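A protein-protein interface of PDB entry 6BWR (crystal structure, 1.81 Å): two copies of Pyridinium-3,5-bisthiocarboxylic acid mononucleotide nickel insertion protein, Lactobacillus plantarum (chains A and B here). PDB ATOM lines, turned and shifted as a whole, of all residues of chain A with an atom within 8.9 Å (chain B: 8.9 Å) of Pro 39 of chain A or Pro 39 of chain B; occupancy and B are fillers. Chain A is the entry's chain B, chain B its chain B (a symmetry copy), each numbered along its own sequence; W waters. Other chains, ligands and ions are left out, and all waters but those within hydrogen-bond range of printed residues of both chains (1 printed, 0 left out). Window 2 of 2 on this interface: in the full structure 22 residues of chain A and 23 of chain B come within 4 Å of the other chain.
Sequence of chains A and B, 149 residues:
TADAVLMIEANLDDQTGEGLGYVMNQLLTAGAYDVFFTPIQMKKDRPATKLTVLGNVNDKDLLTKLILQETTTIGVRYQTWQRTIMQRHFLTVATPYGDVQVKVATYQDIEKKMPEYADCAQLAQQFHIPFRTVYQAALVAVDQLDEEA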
ATOM      1  N   LEU A  12      22.347  36.722 -25.444  1.00  0.00           N
ATOM      2  CA  LEU A  12      22.034  38.077 -25.869  1.00  0.00           C
ATOM      3  C   LEU A  12      20.644  38.437 -25.376  1.00  0.00           C
ATOM      4  O   LEU A  12      19.648  37.915 -25.879  1.00  0.00           O
ATOM      5  CB  LEU A  12      22.138  38.188 -27.385  1.00  0.00           C
ATOM      6  CG  LEU A  12      23.504  37.708 -27.891  1.00  0.00           C
ATOM      7  CD1 LEU A  12      23.420  37.305 -29.331  1.00  0.00           C
ATOM      8  CD2 LEU A  12      24.573  38.762 -27.677  1.00  0.00           C
ATOM      9  N   LEU A  20      19.950  40.219 -35.070  1.00  0.00           N
ATOM     10  CA  LEU A  20      20.411  38.831 -35.017  1.00  0.00           C
ATOM     11  C   LEU A  20      20.396  38.178 -36.393  1.00  0.00           C
ATOM     12  O   LEU A  20      21.289  37.392 -36.720  1.00  0.00           O
ATOM     13  CB  LEU A  20      19.570  38.022 -34.023  1.00  0.00           C
ATOM     14  CG  LEU A  20      19.964  38.253 -32.561  1.00  0.00           C
ATOM     15  CD1 LEU A  20      18.998  37.598 -31.621  1.00  0.00           C
ATOM     16  CD2 LEU A  20      21.353  37.735 -32.330  1.00  0.00           C
ATOM     17  N   PHE A  36      23.341  29.069 -35.210  1.00  0.00           N
ATOM     18  CA  PHE A  36      21.935  28.888 -34.875  1.00  0.00           C
ATOM     19  C   PHE A  36      21.571  29.678 -33.623  1.00  0.00           C
ATOM     20  O   PHE A  36      22.429  30.074 -32.831  1.00  0.00           O
ATOM     21  CB  PHE A  36      21.570  27.399 -34.722  1.00  0.00           C
ATOM     22  CG  PHE A  36      22.345  26.654 -33.668  1.00  0.00           C
ATOM     23  CD1 PHE A  36      23.568  26.065 -33.965  1.00  0.00           C
ATOM     24  CD2 PHE A  36      21.826  26.499 -32.392  1.00  0.00           C
ATOM     25  CE1 PHE A  36      24.271  25.359 -33.000  1.00  0.00           C
ATOM     26  CE2 PHE A  36      22.530  25.794 -31.420  1.00  0.00           C
ATOM     27  CZ  PHE A  36      23.747  25.225 -31.731  1.00  0.00           C
ATOM     28  N   PHE A  37      20.271  29.949 -33.496  1.00  0.00           N
ATOM     29  CA  PHE A  37      19.698  30.667 -32.367  1.00  0.00           C
ATOM     30  C   PHE A  37      18.932  29.700 -31.482  1.00  0.00           C
ATOM     31  O   PHE A  37      18.222  28.826 -31.979  1.00  0.00           O
ATOM     32  CB  PHE A  37      18.748  31.761 -32.838  1.00  0.00           C
ATOM     33  CG  PHE A  37      19.397  32.779 -33.715  1.00  0.00           C
ATOM     34  CD1 PHE A  37      20.574  33.393 -33.330  1.00  0.00           C
ATOM     35  CD2 PHE A  37      18.824  33.138 -34.915  1.00  0.00           C
ATOM     36  CE1 PHE A  37      21.173  34.330 -34.139  1.00  0.00           C
ATOM     37  CE2 PHE A  37      19.421  34.090 -35.724  1.00  0.00           C
ATOM     38  CZ  PHE A  37      20.589  34.681 -35.336  1.00  0.00           C
ATOM     39  N   THR A  38      19.056  29.874 -30.174  1.00  0.00           N
ATOM     40  CA  THR A  38      18.271  29.112 -29.219  1.00  0.00           C
ATOM     41  C   THR A  38      17.506  30.085 -28.343  1.00  0.00           C
ATOM     42  O   THR A  38      18.129  30.918 -27.672  1.00  0.00           O
ATOM     43  CB  THR A  38      19.162  28.227 -28.350  1.00  0.00           C
ATOM     44  OG1 THR A  38      20.004  27.432 -29.174  1.00  0.00           O
ATOM     45  CG2 THR A  38      18.333  27.337 -27.462  1.00  0.00           C
ATOM     46  N   PRO A  39      16.181  30.009 -28.269  1.00  0.00           N
ATOM     47  CA  PRO A  39      15.458  30.874 -27.334  1.00  0.00           C
ATOM     48  C   PRO A  39      15.718  30.456 -25.893  1.00  0.00           C
ATOM     49  O   PRO A  39      15.600  29.285 -25.536  1.00  0.00           O
ATOM     50  CB  PRO A  39      13.996  30.683 -27.738  1.00  0.00           C
ATOM     51  CG  PRO A  39      13.948  29.330 -28.376  1.00  0.00           C
ATOM     52  CD  PRO A  39      15.291  29.086 -29.003  1.00  0.00           C
ATOM     53  N   ILE A  40      16.101  31.425 -25.067  1.00  0.00           N
ATOM     54  CA  ILE A  40      16.402  31.200 -23.663  1.00  0.00           C
ATOM     55  C   ILE A  40      15.688  32.267 -22.853  1.00  0.00           C
ATOM     56  O   ILE A  40      15.220  33.270 -23.382  1.00  0.00           O
ATOM     57  CB  ILE A  40      17.914  31.218 -23.376  1.00  0.00           C
ATOM     58  CG1 ILE A  40      18.514  32.563 -23.742  1.00  0.00           C
ATOM     59  CG2 ILE A  40      18.615  30.109 -24.143  1.00  0.00           C
ATOM     60  CD1 ILE A  40      19.941  32.697 -23.317  1.00  0.00           C
ATOM     61  N   GLN A  41      15.635  32.056 -21.550  1.00  0.00           N
ATOM     62  CA  GLN A  41      14.986  32.975 -20.630  1.00  0.00           C
ATOM     63  C   GLN A  41      16.034  33.458 -19.649  1.00  0.00           C
ATOM     64  O   GLN A  41      16.722  32.647 -19.025  1.00  0.00           O
ATOM     65  CB  GLN A  41      13.831  32.292 -19.905  1.00  0.00           C
ATOM     66  CG  GLN A  41      13.207  33.110 -18.794  1.00  0.00           C
ATOM     67  CD  GLN A  41      11.930  32.479 -18.277  1.00  0.00           C
ATOM     68  OE1 GLN A  41      11.493  31.438 -18.763  1.00  0.00           O
ATOM     69  NE2 GLN A  41      11.310  33.126 -17.311  1.00  0.00           N
ATOM     70  N   MET A  42      16.189  34.760 -19.550  1.00  0.00           N
ATOM     71  CA  MET A  42      17.195  35.327 -18.683  1.00  0.00           C
ATOM     72  C   MET A  42      16.547  36.137 -17.558  1.00  0.00           C
ATOM     73  O   MET A  42      15.325  36.220 -17.421  1.00  0.00           O
ATOM     74  CB  MET A  42      18.189  36.154 -19.502  1.00  0.00           C
ATOM     75  CG  MET A  42      19.068  35.289 -20.353  1.00  0.00           C
ATOM     76  SD  MET A  42      20.237  36.179 -21.366  1.00  0.00           S
ATOM     77  CE  MET A  42      21.340  36.743 -20.086  1.00  0.00           C
ATOM     78  N   ARG A  46      13.414  38.541 -19.086  1.00  0.00           N
ATOM     79  CA  ARG A  46      13.923  38.834 -20.420  1.00  0.00           C
ATOM     80  C   ARG A  46      13.866  37.612 -21.324  1.00  0.00           C
ATOM     81  O   ARG A  46      14.563  36.618 -21.053  1.00  0.00           O
ATOM     82  CB  ARG A  46      15.351  39.358 -20.345  1.00  0.00           C
ATOM     83  CG  ARG A  46      15.453  40.781 -19.826  1.00  0.00           C
ATOM     84  CD  ARG A  46      16.870  41.138 -19.422  1.00  0.00           C
ATOM     85  NE  ARG A  46      16.904  42.410 -18.708  1.00  0.00           N
ATOM     86  CZ  ARG A  46      18.020  42.976 -18.251  1.00  0.00           C
ATOM     87  NH1 ARG A  46      19.195  42.389 -18.446  1.00  0.00           N
ATOM     88  NH2 ARG A  46      17.968  44.123 -17.603  1.00  0.00           N
ATOM     89  N   PRO A  47      13.055  37.627 -22.385  1.00  0.00           N
ATOM     90  CA  PRO A  47      13.179  36.622 -23.434  1.00  0.00           C
ATOM     91  C   PRO A  47      14.418  36.940 -24.252  1.00  0.00           C
ATOM     92  O   PRO A  47      14.517  38.008 -24.853  1.00  0.00           O
ATOM     93  CB  PRO A  47      11.894  36.798 -24.247  1.00  0.00           C
ATOM     94  CG  PRO A  47      11.558  38.213 -24.083  1.00  0.00           C
ATOM     95  CD  PRO A  47      12.087  38.672 -22.754  1.00  0.00           C
ATOM     96  N   ALA A  48      15.386  36.045 -24.220  1.00  0.00           N
ATOM     97  CA  ALA A  48      16.675  36.287 -24.822  1.00  0.00           C
ATOM     98  C   ALA A  48      16.929  35.237 -25.890  1.00  0.00           C
ATOM     99  O   ALA A  48      16.120  34.334 -26.119  1.00  0.00           O
ATOM    100  CB  ALA A  48      17.779  36.269 -23.768  1.00  0.00           C
ATOM    101  N   THR A  49      18.072  35.369 -26.551  1.00  0.00           N
ATOM    102  CA  THR A  49      18.516  34.418 -27.563  1.00  0.00           C
ATOM    103  C   THR A  49      19.952  34.019 -27.271  1.00  0.00           C
ATOM    104  O   THR A  49      20.801  34.884 -27.044  1.00  0.00           O
ATOM    105  CB  THR A  49      18.436  35.011 -28.987  1.00  0.00           C
ATOM    106  OG1 THR A  49      17.081  35.348 -29.313  1.00  0.00           O
ATOM    107  CG2 THR A  49      18.960  34.028 -30.020  1.00  0.00           C
ATOM    108  N   LYS A  50      20.224  32.723 -27.267  1.00  0.00           N
ATOM    109  CA  LYS A  50      21.596  32.245 -27.260  1.00  0.00           C
ATOM    110  C   LYS A  50      22.070  32.091 -28.703  1.00  0.00           C
ATOM    111  O   LYS A  50      21.435  31.399 -29.504  1.00  0.00           O
ATOM    112  CB  LYS A  50      21.731  30.918 -26.520  1.00  0.00           C
ATOM    113  CG  LYS A  50      23.140  30.343 -26.581  1.00  0.00           C
ATOM    114  CD  LYS A  50      23.356  29.159 -25.655  1.00  0.00           C
ATOM    115  CE  LYS A  50      22.766  27.875 -26.188  1.00  0.00           C
ATOM    116  NZ  LYS A  50      23.254  26.702 -25.383  1.00  0.00           N
ATOM    117  N   LEU A  51      23.191  32.726 -29.021  1.00  0.00           N
ATOM    118  CA  LEU A  51      23.827  32.594 -30.320  1.00  0.00           C
ATOM    119  C   LEU A  51      24.900  31.525 -30.220  1.00  0.00           C
ATOM    120  O   LEU A  51      25.803  31.629 -29.387  1.00  0.00           O
ATOM    121  CB  LEU A  51      24.436  33.928 -30.751  1.00  0.00           C
ATOM    122  CG  LEU A  51      25.317  33.996 -31.994  1.00  0.00           C
ATOM    123  CD1 LEU A  51      24.513  33.648 -33.231  1.00  0.00           C
ATOM    124  CD2 LEU A  51      25.910  35.389 -32.119  1.00  0.00           C
ATOM    125  N   THR A  52      24.808  30.497 -31.056  1.00  0.00           N
ATOM    126  CA  THR A  52      25.851  29.483 -31.135  1.00  0.00           C
ATOM    127  C   THR A  52      26.442  29.475 -32.537  1.00  0.00           C
ATOM    128  O   THR A  52      25.718  29.485 -33.534  1.00  0.00           O
ATOM    129  CB  THR A  52      25.322  28.095 -30.764  1.00  0.00           C
ATOM    130  OG1 THR A  52      24.653  28.152 -29.496  1.00  0.00           O
ATOM    131  CG2 THR A  52      26.471  27.111 -30.668  1.00  0.00           C
ATOM    132  N   LEU B  12      15.541  19.435 -16.101  1.00  0.00           N
ATOM    133  CA  LEU B  12      14.529  19.359 -15.058  1.00  0.00           C
ATOM    134  C   LEU B  12      13.181  19.093 -15.703  1.00  0.00           C
ATOM    135  O   LEU B  12      12.618  19.971 -16.359  1.00  0.00           O
ATOM    136  CB  LEU B  12      14.517  20.646 -14.243  1.00  0.00           C
ATOM    137  CG  LEU B  12      15.911  20.975 -13.695  1.00  0.00           C
ATOM    138  CD1 LEU B  12      16.024  22.437 -13.388  1.00  0.00           C
ATOM    139  CD2 LEU B  12      16.238  20.132 -12.477  1.00  0.00           C
ATOM    140  N   LEU B  20      11.386  27.215 -10.370  1.00  0.00           N
ATOM    141  CA  LEU B  20      12.530  27.603 -11.196  1.00  0.00           C
ATOM    142  C   LEU B  20      12.839  29.089 -11.070  1.00  0.00           C
ATOM    143  O   LEU B  20      14.007  29.484 -11.063  1.00  0.00           O
ATOM    144  CB  LEU B  20      12.291  27.221 -12.661  1.00  0.00           C
ATOM    145  CG  LEU B  20      12.532  25.736 -12.950  1.00  0.00           C
ATOM    146  CD1 LEU B  20      12.103  25.369 -14.339  1.00  0.00           C
ATOM    147  CD2 LEU B  20      13.983  25.416 -12.748  1.00  0.00           C
ATOM    148  N   PHE B  36      20.302  30.907 -16.904  1.00  0.00           N
ATOM    149  CA  PHE B  36      19.232  30.996 -17.887  1.00  0.00           C
ATOM    150  C   PHE B  36      18.527  29.654 -18.044  1.00  0.00           C
ATOM    151  O   PHE B  36      19.050  28.598 -17.679  1.00  0.00           O
ATOM    152  CB  PHE B  36      19.741  31.521 -19.243  1.00  0.00           C
ATOM    153  CG  PHE B  36      20.823  30.694 -19.885  1.00  0.00           C
ATOM    154  CD1 PHE B  36      22.162  30.912 -19.582  1.00  0.00           C
ATOM    155  CD2 PHE B  36      20.504  29.733 -20.831  1.00  0.00           C
ATOM    156  CE1 PHE B  36      23.160  30.165 -20.190  1.00  0.00           C
ATOM    157  CE2 PHE B  36      21.504  28.979 -21.441  1.00  0.00           C
ATOM    158  CZ  PHE B  36      22.826  29.202 -21.119  1.00  0.00           C
ATOM    159  N   PHE B  37      17.293  29.729 -18.545  1.00  0.00           N
ATOM    160  CA  PHE B  37      16.450  28.572 -18.804  1.00  0.00           C
ATOM    161  C   PHE B  37      16.357  28.331 -20.300  1.00  0.00           C
ATOM    162  O   PHE B  37      16.227  29.274 -21.078  1.00  0.00           O
ATOM    163  CB  PHE B  37      15.046  28.782 -18.251  1.00  0.00           C
ATOM    164  CG  PHE B  37      15.013  29.022 -16.779  1.00  0.00           C
ATOM    165  CD1 PHE B  37      15.673  28.173 -15.912  1.00  0.00           C
ATOM    166  CD2 PHE B  37      14.307  30.084 -16.257  1.00  0.00           C
ATOM    167  CE1 PHE B  37      15.645  28.396 -14.555  1.00  0.00           C
ATOM    168  CE2 PHE B  37      14.268  30.302 -14.891  1.00  0.00           C
ATOM    169  CZ  PHE B  37      14.934  29.461 -14.046  1.00  0.00           C
ATOM    170  N   THR B  38      16.399  27.066 -20.697  1.00  0.00           N
ATOM    171  CA  THR B  38      16.180  26.688 -22.081  1.00  0.00           C
ATOM    172  C   THR B  38      15.030  25.700 -22.132  1.00  0.00           C
ATOM    173  O   THR B  38      15.115  24.636 -21.505  1.00  0.00           O
ATOM    174  CB  THR B  38      17.431  26.054 -22.686  1.00  0.00           C
ATOM    175  OG1 THR B  38      18.550  26.908 -22.489  1.00  0.00           O
ATOM    176  CG2 THR B  38      17.244  25.794 -24.158  1.00  0.00           C
ATOM    177  N   PRO B  39      13.964  25.963 -22.879  1.00  0.00           N
ATOM    178  CA  PRO B  39      12.909  24.956 -23.016  1.00  0.00           C
ATOM    179  C   PRO B  39      13.391  23.772 -23.845  1.00  0.00           C
ATOM    180  O   PRO B  39      13.940  23.935 -24.934  1.00  0.00           O
ATOM    181  CB  PRO B  39      11.779  25.722 -23.703  1.00  0.00           C
ATOM    182  CG  PRO B  39      12.460  26.829 -24.444  1.00  0.00           C
ATOM    183  CD  PRO B  39      13.703  27.179 -23.678  1.00  0.00           C
ATOM    184  N   ILE B  40      13.205  22.571 -23.305  1.00  0.00           N
ATOM    185  CA  ILE B  40      13.615  21.337 -23.953  1.00  0.00           C
ATOM    186  C   ILE B  40      12.454  20.360 -23.880  1.00  0.00           C
ATOM    187  O   ILE B  40      11.503  20.549 -23.130  1.00  0.00           O
ATOM    188  CB  ILE B  40      14.879  20.731 -23.319  1.00  0.00           C
ATOM    189  CG1 ILE B  40      14.639  20.399 -21.857  1.00  0.00           C
ATOM    190  CG2 ILE B  40      16.052  21.689 -23.450  1.00  0.00           C
ATOM    191  CD1 ILE B  40      15.773  19.645 -21.240  1.00  0.00           C
ATOM    192  N   GLN B  41      12.558  19.290 -24.649  1.00  0.00           N
ATOM    193  CA  GLN B  41      11.536  18.258 -24.701  1.00  0.00           C
ATOM    194  C   GLN B  41      12.175  16.957 -24.263  1.00  0.00           C
ATOM    195  O   GLN B  41      13.210  16.560 -24.804  1.00  0.00           O
ATOM    196  CB  GLN B  41      10.959  18.138 -26.107  1.00  0.00           C
ATOM    197  CG  GLN B  41      10.018  16.969 -26.309  1.00  0.00           C
ATOM    198  CD  GLN B  41       9.304  17.042 -27.644  1.00  0.00           C
ATOM    199  OE1 GLN B  41       9.494  17.980 -28.416  1.00  0.00           O
ATOM    200  NE2 GLN B  41       8.456  16.068 -27.906  1.00  0.00           N
ATOM    201  N   MET B  42      11.598  16.328 -23.263  1.00  0.00           N
ATOM    202  CA  MET B  42      12.153  15.105 -22.732  1.00  0.00           C
ATOM    203  C   MET B  42      11.196  13.932 -22.957  1.00  0.00           C
ATOM    204  O   MET B  42      10.130  14.054 -23.564  1.00  0.00           O
ATOM    205  CB  MET B  42      12.515  15.290 -21.256  1.00  0.00           C
ATOM    206  CG  MET B  42      13.701  16.187 -21.080  1.00  0.00           C
ATOM    207  SD  MET B  42      14.171  16.482 -19.383  1.00  0.00           S
ATOM    208  CE  MET B  42      14.819  14.870 -18.991  1.00  0.00           C
ATOM    209  N   ARG B  46       7.223  15.072 -22.042  1.00  0.00           N
ATOM    210  CA  ARG B  46       7.455  16.034 -20.972  1.00  0.00           C
ATOM    211  C   ARG B  46       8.052  17.330 -21.502  1.00  0.00           C
ATOM    212  O   ARG B  46       9.185  17.316 -22.015  1.00  0.00           O
ATOM    213  CB  ARG B  46       8.368  15.440 -19.908  1.00  0.00           C
ATOM    214  CG  ARG B  46       7.691  14.400 -19.033  1.00  0.00           C
ATOM    215  CD  ARG B  46       8.694  13.580 -18.246  1.00  0.00           C
ATOM    216  NE  ARG B  46       8.047  12.440 -17.605  1.00  0.00           N
ATOM    217  CZ  ARG B  46       8.685  11.559 -16.835  1.00  0.00           C
ATOM    218  NH1 ARG B  46       9.984  11.696 -16.600  1.00  0.00           N
ATOM    219  NH2 ARG B  46       8.032  10.546 -16.300  1.00  0.00           N
ATOM    220  N   PRO B  47       7.338  18.454 -21.417  1.00  0.00           N
ATOM    221  CA  PRO B  47       7.964  19.754 -21.630  1.00  0.00           C
ATOM    222  C   PRO B  47       8.808  20.081 -20.412  1.00  0.00           C
ATOM    223  O   PRO B  47       8.294  20.179 -19.299  1.00  0.00           O
ATOM    224  CB  PRO B  47       6.771  20.702 -21.773  1.00  0.00           C
ATOM    225  CG  PRO B  47       5.722  20.083 -20.963  1.00  0.00           C
ATOM    226  CD  PRO B  47       5.948  18.597 -20.956  1.00  0.00           C
ATOM    227  N   ALA B  48      10.108  20.181 -20.610  1.00  0.00           N
ATOM    228  CA  ALA B  48      11.041  20.332 -19.520  1.00  0.00           C
ATOM    229  C   ALA B  48      11.800  21.637 -19.693  1.00  0.00           C
ATOM    230  O   ALA B  48      11.608  22.375 -20.663  1.00  0.00           O
ATOM    231  CB  ALA B  48      12.002  19.148 -19.458  1.00  0.00           C
ATOM    232  N   THR B  49      12.669  21.918 -18.731  1.00  0.00           N
ATOM    233  CA  THR B  49      13.534  23.090 -18.762  1.00  0.00           C
ATOM    234  C   THR B  49      14.962  22.660 -18.477  1.00  0.00           C
ATOM    235  O   THR B  49      15.208  21.928 -17.515  1.00  0.00           O
ATOM    236  CB  THR B  49      13.108  24.149 -17.722  1.00  0.00           C
ATOM    237  OG1 THR B  49      11.781  24.617 -17.998  1.00  0.00           O
ATOM    238  CG2 THR B  49      14.058  25.335 -17.728  1.00  0.00           C
ATOM    239  N   LYS B  50      15.896  23.098 -19.306  1.00  0.00           N
ATOM    240  CA  LYS B  50      17.307  22.967 -18.983  1.00  0.00           C
ATOM    241  C   LYS B  50      17.752  24.208 -18.214  1.00  0.00           C
ATOM    242  O   LYS B  50      17.578  25.337 -18.683  1.00  0.00           O
ATOM    243  CB  LYS B  50      18.163  22.792 -20.234  1.00  0.00           C
ATOM    244  CG  LYS B  50      19.655  22.751 -19.934  1.00  0.00           C
ATOM    245  CD  LYS B  50      20.505  22.335 -21.122  1.00  0.00           C
ATOM    246  CE  LYS B  50      20.697  23.443 -22.129  1.00  0.00           C
ATOM    247  NZ  LYS B  50      21.766  23.070 -23.119  1.00  0.00           N
ATOM    248  N   LEU B  51      18.338  23.992 -17.042  1.00  0.00           N
ATOM    249  CA  LEU B  51      18.910  25.059 -16.241  1.00  0.00           C
ATOM    250  C   LEU B  51      20.394  25.143 -16.547  1.00  0.00           C
ATOM    251  O   LEU B  51      21.115  24.154 -16.395  1.00  0.00           O
ATOM    252  CB  LEU B  51      18.682  24.788 -14.754  1.00  0.00           C
ATOM    253  CG  LEU B  51      19.352  25.672 -13.707  1.00  0.00           C
ATOM    254  CD1 LEU B  51      18.838  27.094 -13.810  1.00  0.00           C
ATOM    255  CD2 LEU B  51      19.087  25.108 -12.322  1.00  0.00           C
ATOM    256  N   THR B  52      20.857  26.311 -16.981  1.00  0.00           N
ATOM    257  CA  THR B  52      22.281  26.539 -17.180  1.00  0.00           C
ATOM    258  C   THR B  52      22.746  27.660 -16.263  1.00  0.00           C
ATOM    259  O   THR B  52      22.110  28.710 -16.168  1.00  0.00           O
ATOM    260  CB  THR B  52      22.604  26.867 -18.641  1.00  0.00           C
ATOM    261  OG1 THR B  52      22.045  25.863 -19.500  1.00  0.00           O
ATOM    262  CG2 THR B  52      24.106  26.903 -18.844  1.00  0.00           C
HETATM  263  O   HOH W   1      20.699  25.915 -24.197  1.00  0.00           O
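Pro 39 of chain A touches just one residue of chain B: Pro 39 (3.4 Å).
Of chain A, only Pro 39 comes within 4 Å of Pro 39 of chain B.
Of chain B, only Thr 38 comes within 4 Å of Thr 38 of chain A.
Of chain A, only Thr 38 (3.8 Å) and Ile 40 (3.6 Å) come within 4 Å of Thr 38 of chain B.
Of the printed residues of chain A, Phe 37 of chain B touches Ile 40 and Gln 41.
Of the printed residues of chain B, Ile 40 of chain A touches Phe 36 (3.8 Å), Phe 37 (3.2 Å) and Thr 38 (3.6 Å).
Water W1 lies within hydrogen-bond range of OG1 of Thr 38 of chain B (2.9 Å), NZ of Lys 50 of chain A (2.9 Å) and NZ of Lys 50 of chain B (3.2 Å).
The backbone NH (N) of Lys 50 of chain B lies within hydrogen-bond range of the backbone carbonyl oxygen (O) of Thr 38 of chain B (2.8 Å).
O of Thr 38 of chain A is in hydrogen-bond range of N of Lys 50 of chain A, 2.8 Å away.
O of Thr 52 of chain B is in hydrogen-bond range of N of Phe 36 of chain B, at 2.9 Å.
N of Ala 48 of chain A is in hydrogen-bond range of O of Ile 40 of chain A (2.9 Å).
Thr 38 of chain A touches Thr 38 of chain B.
Pro 39 of chain A touches Pro 39 of chain B (O to CD, 3.4 Å).
Ile 40 of chain A touches Phe 36 of chain B (CG2 to CD2, 3.8 Å).
Ile 40 of chain A touches Phe 37 of chain B.
Ile 40 of chain A touches Thr 38 of chain B (CG2 to OG1, 3.6 Å).
Gln 41 of chain A touches Phe 36 of chain B.
Met 42 of chain A touches Phe 36 of chain B (CG to CB, 3.99 Å).
O of Phe 37 of chain B is in hydrogen-bond range of N of Gln 41 of chain A (2.9 Å).
Hydrophobic or aromatic side chains of chain A that line the printed part of chain B: Ile 40 and Met 42.
Along chain A the printed residues that touch a printed residue of chain B span positions 38 to 42.
Of the 16 printed residues of chain B, 4 touch a printed residue of chain A.
Hydrophobic or aromatic side chains of chain B within 4 Å of the printed part of chain A: Phe 36, Phe 37 and Pro 39.
Among the printed residues, 8 pairs touch across the chains.
Pro 39 of chain A touches its own counterpart, Pro 39 of chain B.
Ile 40 of chain A touches Phe 37 of chain B, but with the chains exchanged Phe 37 of chain A does not touch Ile 40 of chain B (11.3 Å).
Ile 40 of chain A touches Thr 38 of chain B, but with the chains exchanged Thr 38 of chain A does not touch Ile 40 of chain B (7.3 Å).
Gln 41 of chain A touches Phe 36 of chain B, but with the chains exchanged Phe 36 of chain A does not touch Gln 41 of chain B (13.7 Å).
Positions printed for both chains: 12, 20, 36, 37, 38, 39, 40, 41, 42, 46, 47, 48, 49, 50, 51 and 52.
Of the 8 pairs that touch across the chains among the printed residues, 2 have their exchanged pair printed and touching as well.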
